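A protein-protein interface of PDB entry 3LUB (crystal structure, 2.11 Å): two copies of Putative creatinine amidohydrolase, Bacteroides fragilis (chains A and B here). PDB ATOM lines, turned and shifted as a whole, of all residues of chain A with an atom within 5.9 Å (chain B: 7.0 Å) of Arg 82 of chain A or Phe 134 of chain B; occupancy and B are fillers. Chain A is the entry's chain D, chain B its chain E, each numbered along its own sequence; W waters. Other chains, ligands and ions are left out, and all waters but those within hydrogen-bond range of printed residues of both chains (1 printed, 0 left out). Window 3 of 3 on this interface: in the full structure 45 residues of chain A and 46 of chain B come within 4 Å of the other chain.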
ATOM      1  N   HIS A  77      -2.902  17.848   5.250  1.00  0.00           N
ATOM      2  CA  HIS A  77      -2.435  18.737   4.200  1.00  0.00           C
ATOM      3  C   HIS A  77      -0.932  18.599   3.848  1.00  0.00           C
ATOM      4  O   HIS A  77      -0.208  17.795   4.433  1.00  0.00           O
ATOM      5  CB  HIS A  77      -2.892  20.175   4.512  1.00  0.00           C
ATOM      6  CG  HIS A  77      -4.391  20.308   4.511  1.00  0.00           C
ATOM      7  ND1 HIS A  77      -5.142  20.112   3.379  1.00  0.00           N
ATOM      8  CD2 HIS A  77      -5.279  20.452   5.521  1.00  0.00           C
ATOM      9  CE1 HIS A  77      -6.426  20.207   3.673  1.00  0.00           C
ATOM     10  NE2 HIS A  77      -6.535  20.406   4.970  1.00  0.00           N
ATOM     11  N   ASN A  78      -0.520  19.314   2.813  1.00  0.00           N
ATOM     12  CA  ASN A  78       0.784  19.121   2.165  1.00  0.00           C
ATOM     13  C   ASN A  78       1.697  20.257   2.569  1.00  0.00           C
ATOM     14  O   ASN A  78       1.217  21.288   3.051  1.00  0.00           O
ATOM     15  CB  ASN A  78       0.649  19.151   0.623  1.00  0.00           C
ATOM     16  CG  ASN A  78       0.122  17.837   0.025  1.00  0.00           C
ATOM     17  OD1 ASN A  78      -0.561  17.063   0.682  1.00  0.00           O
ATOM     18  ND2 ASN A  78       0.462  17.592  -1.236  1.00  0.00           N
ATOM     19  N   PRO A  79       3.017  20.092   2.360  1.00  0.00           N
ATOM     20  CA  PRO A  79       3.855  21.252   2.589  1.00  0.00           C
ATOM     21  C   PRO A  79       3.430  22.435   1.680  1.00  0.00           C
ATOM     22  O   PRO A  79       2.969  22.241   0.551  1.00  0.00           O
ATOM     23  CB  PRO A  79       5.278  20.727   2.318  1.00  0.00           C
ATOM     24  CG  PRO A  79       5.182  19.227   2.397  1.00  0.00           C
ATOM     25  CD  PRO A  79       3.802  18.910   1.930  1.00  0.00           C
ATOM     26  N   GLY A  80       3.522  23.637   2.230  1.00  0.00           N
ATOM     27  CA  GLY A  80       3.059  24.856   1.561  1.00  0.00           C
ATOM     28  C   GLY A  80       1.626  25.267   1.848  1.00  0.00           C
ATOM     29  O   GLY A  80       1.276  26.428   1.662  1.00  0.00           O
ATOM     30  N   GLN A  81       0.800  24.318   2.297  1.00  0.00           N
ATOM     31  CA  GLN A  81      -0.607  24.590   2.546  1.00  0.00           C
ATOM     32  C   GLN A  81      -0.794  25.162   3.933  1.00  0.00           C
ATOM     33  O   GLN A  81      -1.641  26.026   4.132  1.00  0.00           O
ATOM     34  CB  GLN A  81      -1.467  23.343   2.414  1.00  0.00           C
ATOM     35  CG  GLN A  81      -1.501  22.763   1.019  1.00  0.00           C
ATOM     36  CD  GLN A  81      -2.666  21.862   0.809  1.00  0.00           C
ATOM     37  OE1 GLN A  81      -2.614  20.671   1.130  1.00  0.00           O
ATOM     38  NE2 GLN A  81      -3.751  22.417   0.266  1.00  0.00           N
ATOM     39  N   ARG A  82       0.010  24.697   4.882  1.00  0.00           N
ATOM     40  CA  ARG A  82      -0.139  25.087   6.287  1.00  0.00           C
ATOM     41  C   ARG A  82       0.118  26.599   6.502  1.00  0.00           C
ATOM     42  O   ARG A  82      -0.411  27.200   7.426  1.00  0.00           O
ATOM     43  CB  ARG A  82       0.816  24.265   7.149  1.00  0.00           C
ATOM     44  CG  ARG A  82       0.521  24.338   8.620  1.00  0.00           C
ATOM     45  CD  ARG A  82       1.364  23.335   9.412  1.00  0.00           C
ATOM     46  NE  ARG A  82       2.787  23.658   9.285  1.00  0.00           N
ATOM     47  CZ  ARG A  82       3.737  23.268  10.132  1.00  0.00           C
ATOM     48  NH1 ARG A  82       3.430  22.554  11.189  1.00  0.00           N
ATOM     49  NH2 ARG A  82       5.005  23.607   9.929  1.00  0.00           N
ATOM     50  N   GLU A  83       0.934  27.177   5.630  1.00  0.00           N
ATOM     51  CA  GLU A  83       1.329  28.568   5.716  1.00  0.00           C
ATOM     52  C   GLU A  83       0.268  29.525   5.117  1.00  0.00           C
ATOM     53  O   GLU A  83       0.303  30.734   5.363  1.00  0.00           O
ATOM     54  CB  GLU A  83       2.719  28.743   5.070  1.00  0.00           C
ATOM     55  CG  GLU A  83       2.830  28.472   3.537  1.00  0.00           C
ATOM     56  CD  GLU A  83       4.312  28.419   3.003  1.00  0.00           C
ATOM     57  OE1 GLU A  83       5.037  27.411   3.269  1.00  0.00           O
ATOM     58  OE2 GLU A  83       4.749  29.392   2.323  1.00  0.00           O
ATOM     59  N   LEU A  84      -0.680  28.972   4.354  1.00  0.00           N
ATOM     60  CA  LEU A  84      -1.797  29.742   3.799  1.00  0.00           C
ATOM     61  C   LEU A  84      -2.762  30.059   4.942  1.00  0.00           C
ATOM     62  O   LEU A  84      -3.017  29.188   5.771  1.00  0.00           O
ATOM     63  CB  LEU A  84      -2.508  28.958   2.697  1.00  0.00           C
ATOM     64  CG  LEU A  84      -1.746  28.712   1.374  1.00  0.00           C
ATOM     65  CD1 LEU A  84      -2.552  27.770   0.487  1.00  0.00           C
ATOM     66  CD2 LEU A  84      -1.369  30.013   0.638  1.00  0.00           C
ATOM     67  N   PRO A  85      -3.296  31.296   4.995  1.00  0.00           N
ATOM     68  CA  PRO A  85      -4.125  31.666   6.124  1.00  0.00           C
ATOM     69  C   PRO A  85      -5.333  30.749   6.322  1.00  0.00           C
ATOM     70  O   PRO A  85      -6.057  30.444   5.392  1.00  0.00           O
ATOM     71  CB  PRO A  85      -4.558  33.091   5.786  1.00  0.00           C
ATOM     72  CG  PRO A  85      -4.389  33.208   4.369  1.00  0.00           C
ATOM     73  CD  PRO A  85      -3.215  32.392   4.033  1.00  0.00           C
ATOM     74  N   CYS A  87      -5.669  27.616   6.865  1.00  0.00           N
ATOM     75  CA  CYS A  87      -5.545  26.214   6.526  1.00  0.00           C
ATOM     76  C   CYS A  87      -5.057  25.436   7.755  1.00  0.00           C
ATOM     77  O   CYS A  87      -4.032  25.742   8.358  1.00  0.00           O
ATOM     78  CB  CYS A  87      -4.546  26.013   5.370  1.00  0.00           C
ATOM     79  SG  CYS A  87      -4.369  24.290   4.843  1.00  0.00           S
ATOM     80  N   HIS A  89      -3.838  21.982   9.182  1.00  0.00           N
ATOM     81  CA  HIS A  89      -3.302  20.661   9.002  1.00  0.00           C
ATOM     82  C   HIS A  89      -3.572  19.821  10.235  1.00  0.00           C
ATOM     83  O   HIS A  89      -3.268  20.234  11.311  1.00  0.00           O
ATOM     84  CB  HIS A  89      -1.794  20.696   8.774  1.00  0.00           C
ATOM     85  CG  HIS A  89      -1.186  19.331   8.763  1.00  0.00           C
ATOM     86  ND1 HIS A  89      -1.525  18.387   7.818  1.00  0.00           N
ATOM     87  CD2 HIS A  89      -0.312  18.729   9.610  1.00  0.00           C
ATOM     88  CE1 HIS A  89      -0.848  17.276   8.058  1.00  0.00           C
ATOM     89  NE2 HIS A  89      -0.120  17.452   9.149  1.00  0.00           N
ATOM     90  N   ILE B 129       4.219  10.466   6.084  1.00  0.00           N
ATOM     91  CA  ILE B 129       5.101  11.368   5.325  1.00  0.00           C
ATOM     92  C   ILE B 129       4.680  12.836   5.412  1.00  0.00           C
ATOM     93  O   ILE B 129       5.522  13.710   5.551  1.00  0.00           O
ATOM     94  CB  ILE B 129       5.219  10.899   3.848  1.00  0.00           C
ATOM     95  CG1 ILE B 129       6.111   9.670   3.780  1.00  0.00           C
ATOM     96  CG2 ILE B 129       5.780  11.984   2.940  1.00  0.00           C
ATOM     97  CD1 ILE B 129       5.980   8.926   2.452  1.00  0.00           C
ATOM     98  N   ARG B 130       3.383  13.115   5.349  1.00  0.00           N
ATOM     99  CA  ARG B 130       2.883  14.486   5.534  1.00  0.00           C
ATOM    100  C   ARG B 130       3.254  15.013   6.924  1.00  0.00           C
ATOM    101  O   ARG B 130       3.728  16.127   7.065  1.00  0.00           O
ATOM    102  CB  ARG B 130       1.370  14.542   5.379  1.00  0.00           C
ATOM    103  CG  ARG B 130       0.914  14.374   3.963  1.00  0.00           C
ATOM    104  CD  ARG B 130      -0.606  14.380   3.830  1.00  0.00           C
ATOM    105  NE  ARG B 130      -0.957  14.698   2.457  1.00  0.00           N
ATOM    106  CZ  ARG B 130      -1.415  13.843   1.547  1.00  0.00           C
ATOM    107  NH1 ARG B 130      -1.664  12.585   1.826  1.00  0.00           N
ATOM    108  NH2 ARG B 130      -1.672  14.289   0.341  1.00  0.00           N
ATOM    109  N   ASP B 131       3.016  14.211   7.955  1.00  0.00           N
ATOM    110  CA  ASP B 131       3.363  14.618   9.307  1.00  0.00           C
ATOM    111  C   ASP B 131       4.865  14.872   9.500  1.00  0.00           C
ATOM    112  O   ASP B 131       5.251  15.845  10.147  1.00  0.00           O
ATOM    113  CB  ASP B 131       2.798  13.611  10.306  1.00  0.00           C
ATOM    114  CG  ASP B 131       1.270  13.637  10.347  1.00  0.00           C
ATOM    115  OD1 ASP B 131       0.678  14.598   9.811  1.00  0.00           O
ATOM    116  OD2 ASP B 131       0.650  12.716  10.931  1.00  0.00           O
ATOM    117  N   LEU B 132       5.711  14.041   8.905  1.00  0.00           N
ATOM    118  CA  LEU B 132       7.155  14.250   9.015  1.00  0.00           C
ATOM    119  C   LEU B 132       7.693  15.390   8.146  1.00  0.00           C
ATOM    120  O   LEU B 132       8.740  15.941   8.429  1.00  0.00           O
ATOM    121  CB  LEU B 132       7.913  12.972   8.718  1.00  0.00           C
ATOM    122  CG  LEU B 132       7.843  11.933   9.825  1.00  0.00           C
ATOM    123  CD1 LEU B 132       8.097  10.543   9.221  1.00  0.00           C
ATOM    124  CD2 LEU B 132       8.821  12.249  10.906  1.00  0.00           C
ATOM    125  N   ALA B 133       6.975  15.725   7.082  1.00  0.00           N
ATOM    126  CA  ALA B 133       7.330  16.856   6.246  1.00  0.00           C
ATOM    127  C   ALA B 133       7.322  18.132   7.047  1.00  0.00           C
ATOM    128  O   ALA B 133       8.096  18.998   6.770  1.00  0.00           O
ATOM    129  CB  ALA B 133       6.377  16.970   5.047  1.00  0.00           C
ATOM    130  N   PHE B 134       6.440  18.230   8.039  1.00  0.00           N
ATOM    131  CA  PHE B 134       6.337  19.403   8.904  1.00  0.00           C
ATOM    132  C   PHE B 134       7.348  19.392  10.032  1.00  0.00           C
ATOM    133  O   PHE B 134       7.880  20.435  10.367  1.00  0.00           O
ATOM    134  CB  PHE B 134       4.892  19.573   9.427  1.00  0.00           C
ATOM    135  CG  PHE B 134       3.880  19.866   8.322  1.00  0.00           C
ATOM    136  CD1 PHE B 134       4.043  20.953   7.475  1.00  0.00           C
ATOM    137  CD2 PHE B 134       2.805  19.055   8.114  1.00  0.00           C
ATOM    138  CE1 PHE B 134       3.128  21.193   6.449  1.00  0.00           C
ATOM    139  CE2 PHE B 134       1.885  19.307   7.087  1.00  0.00           C
ATOM    140  CZ  PHE B 134       2.042  20.361   6.274  1.00  0.00           C
ATOM    141  N   GLU B 135       7.631  18.217  10.606  1.00  0.00           N
ATOM    142  CA  GLU B 135       8.690  18.086  11.624  1.00  0.00           C
ATOM    143  C   GLU B 135      10.097  18.259  11.063  1.00  0.00           C
ATOM    144  O   GLU B 135      10.978  18.763  11.749  1.00  0.00           O
ATOM    145  CB  GLU B 135       8.668  16.706  12.291  1.00  0.00           C
ATOM    146  CG  GLU B 135       7.415  16.337  13.075  1.00  0.00           C
ATOM    147  CD  GLU B 135       7.522  14.911  13.671  1.00  0.00           C
ATOM    148  OE1 GLU B 135       6.712  14.022  13.269  1.00  0.00           O
ATOM    149  OE2 GLU B 135       8.429  14.681  14.521  1.00  0.00           O
ATOM    150  N   TYR B 136      10.332  17.734   9.864  1.00  0.00           N
ATOM    151  CA  TYR B 136      11.673  17.734   9.239  1.00  0.00           C
ATOM    152  C   TYR B 136      11.526  18.301   7.838  1.00  0.00           C
ATOM    153  O   TYR B 136      11.520  17.552   6.854  1.00  0.00           O
ATOM    154  CB  TYR B 136      12.269  16.317   9.155  1.00  0.00           C
ATOM    155  CG  TYR B 136      12.452  15.617  10.488  1.00  0.00           C
ATOM    156  CD1 TYR B 136      13.601  15.801  11.233  1.00  0.00           C
ATOM    157  CD2 TYR B 136      11.465  14.768  10.995  1.00  0.00           C
ATOM    158  CE1 TYR B 136      13.759  15.182  12.463  1.00  0.00           C
ATOM    159  CE2 TYR B 136      11.611  14.138  12.225  1.00  0.00           C
ATOM    160  CZ  TYR B 136      12.766  14.346  12.955  1.00  0.00           C
ATOM    161  OH  TYR B 136      12.944  13.718  14.176  1.00  0.00           O
ATOM    162  N   PRO B 137      11.344  19.626   7.732  1.00  0.00           N
ATOM    163  CA  PRO B 137      11.081  20.260   6.432  1.00  0.00           C
ATOM    164  C   PRO B 137      12.184  20.052   5.393  1.00  0.00           C
ATOM    165  O   PRO B 137      11.920  20.166   4.188  1.00  0.00           O
ATOM    166  CB  PRO B 137      10.944  21.754   6.786  1.00  0.00           C
ATOM    167  CG  PRO B 137      11.494  21.903   8.122  1.00  0.00           C
ATOM    168  CD  PRO B 137      11.350  20.611   8.830  1.00  0.00           C
HETATM  169  O   HOH W   1       2.706  17.493   4.563  1.00  0.00           O
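Water W1 bridges the backbone carbonyl oxygen of His 77 of chain A (2.9 Å) and the backbone carbonyl oxygen of Arg 130 of chain B (3.0 Å).
His 77 of chain A touches Arg 130 of chain B. His 77 of chain A touches Phe 134 of chain B (O to CE2, 3.7 Å). O of Asn 78 of chain A touches CZ of Phe 134 of chain B, 3.5 Å away. Ala 133 of chain B touches Pro 79 of chain A. CA of Pro 79 of chain A touches CE1 of Phe 134 of chain B, at 3.9 Å. Arg 82 of chain A touches Phe 134 of chain B (NE to CD1, 3.5 Å). CD2 of His 89 of chain A touches CE2 of Phe 134 of chain B, at 3.4 Å.
No position is printed for both chains. Of the 9 pairs that touch across the chains among the printed residues, none has its exchanged pair printed and touching as well.
Of the 11 printed residues of chain A, 5 touch a printed residue of chain B. Hydrophobic or aromatic side chains of chain A within 4 Å of the printed part of chain B: Pro 79 and His 89. Along chain A the printed residues that touch a printed residue of chain B span positions 77 to 89. Of the 9 printed residues of chain B, 4 touch a printed residue of chain A. Hydrophobic or aromatic side chains of chain B within 4 Å of the printed part of chain A: Ala 133 and Phe 134. Along chain B the printed residues that touch a printed residue of chain A span positions 130 to 134.
Of chain B, only Phe 134 (3.5 Å) comes within 4 Å of Arg 82 of chain A. Of chain A, only His 77, Asn 78, Pro 79, Arg 82 and His 89 come within 4 Å of Phe 134 of chain B. Of the printed residues of chain B, His 89 of chain A touches Asp 131 and Phe 134. Of the printed residues of chain A, Ala 133 of chain B touches Pro 79.
The side-chain amide oxygen of Gln 81 of chain A sits close to a ring nitrogen (ND1) of His 77 of chain A. The backbone NH of His 77 of chain A sits at hydrogen-bond distance from a ring nitrogen (ND1) of His 89 of chain A, at 3.0 Å. N of Asn 78 of chain A is in hydrogen-bond range of OE1 of Gln 81 of chain A, 3.0 Å away.
The guanidinium group of Arg 130 of chain B sits at hydrogen-bond distance from the side-chain amide oxygen of Asn 78 of chain A (3.0 Å). NE2 of His 89 of chain A lies within hydrogen-bond range of OD1 of Asp 131 of chain B.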
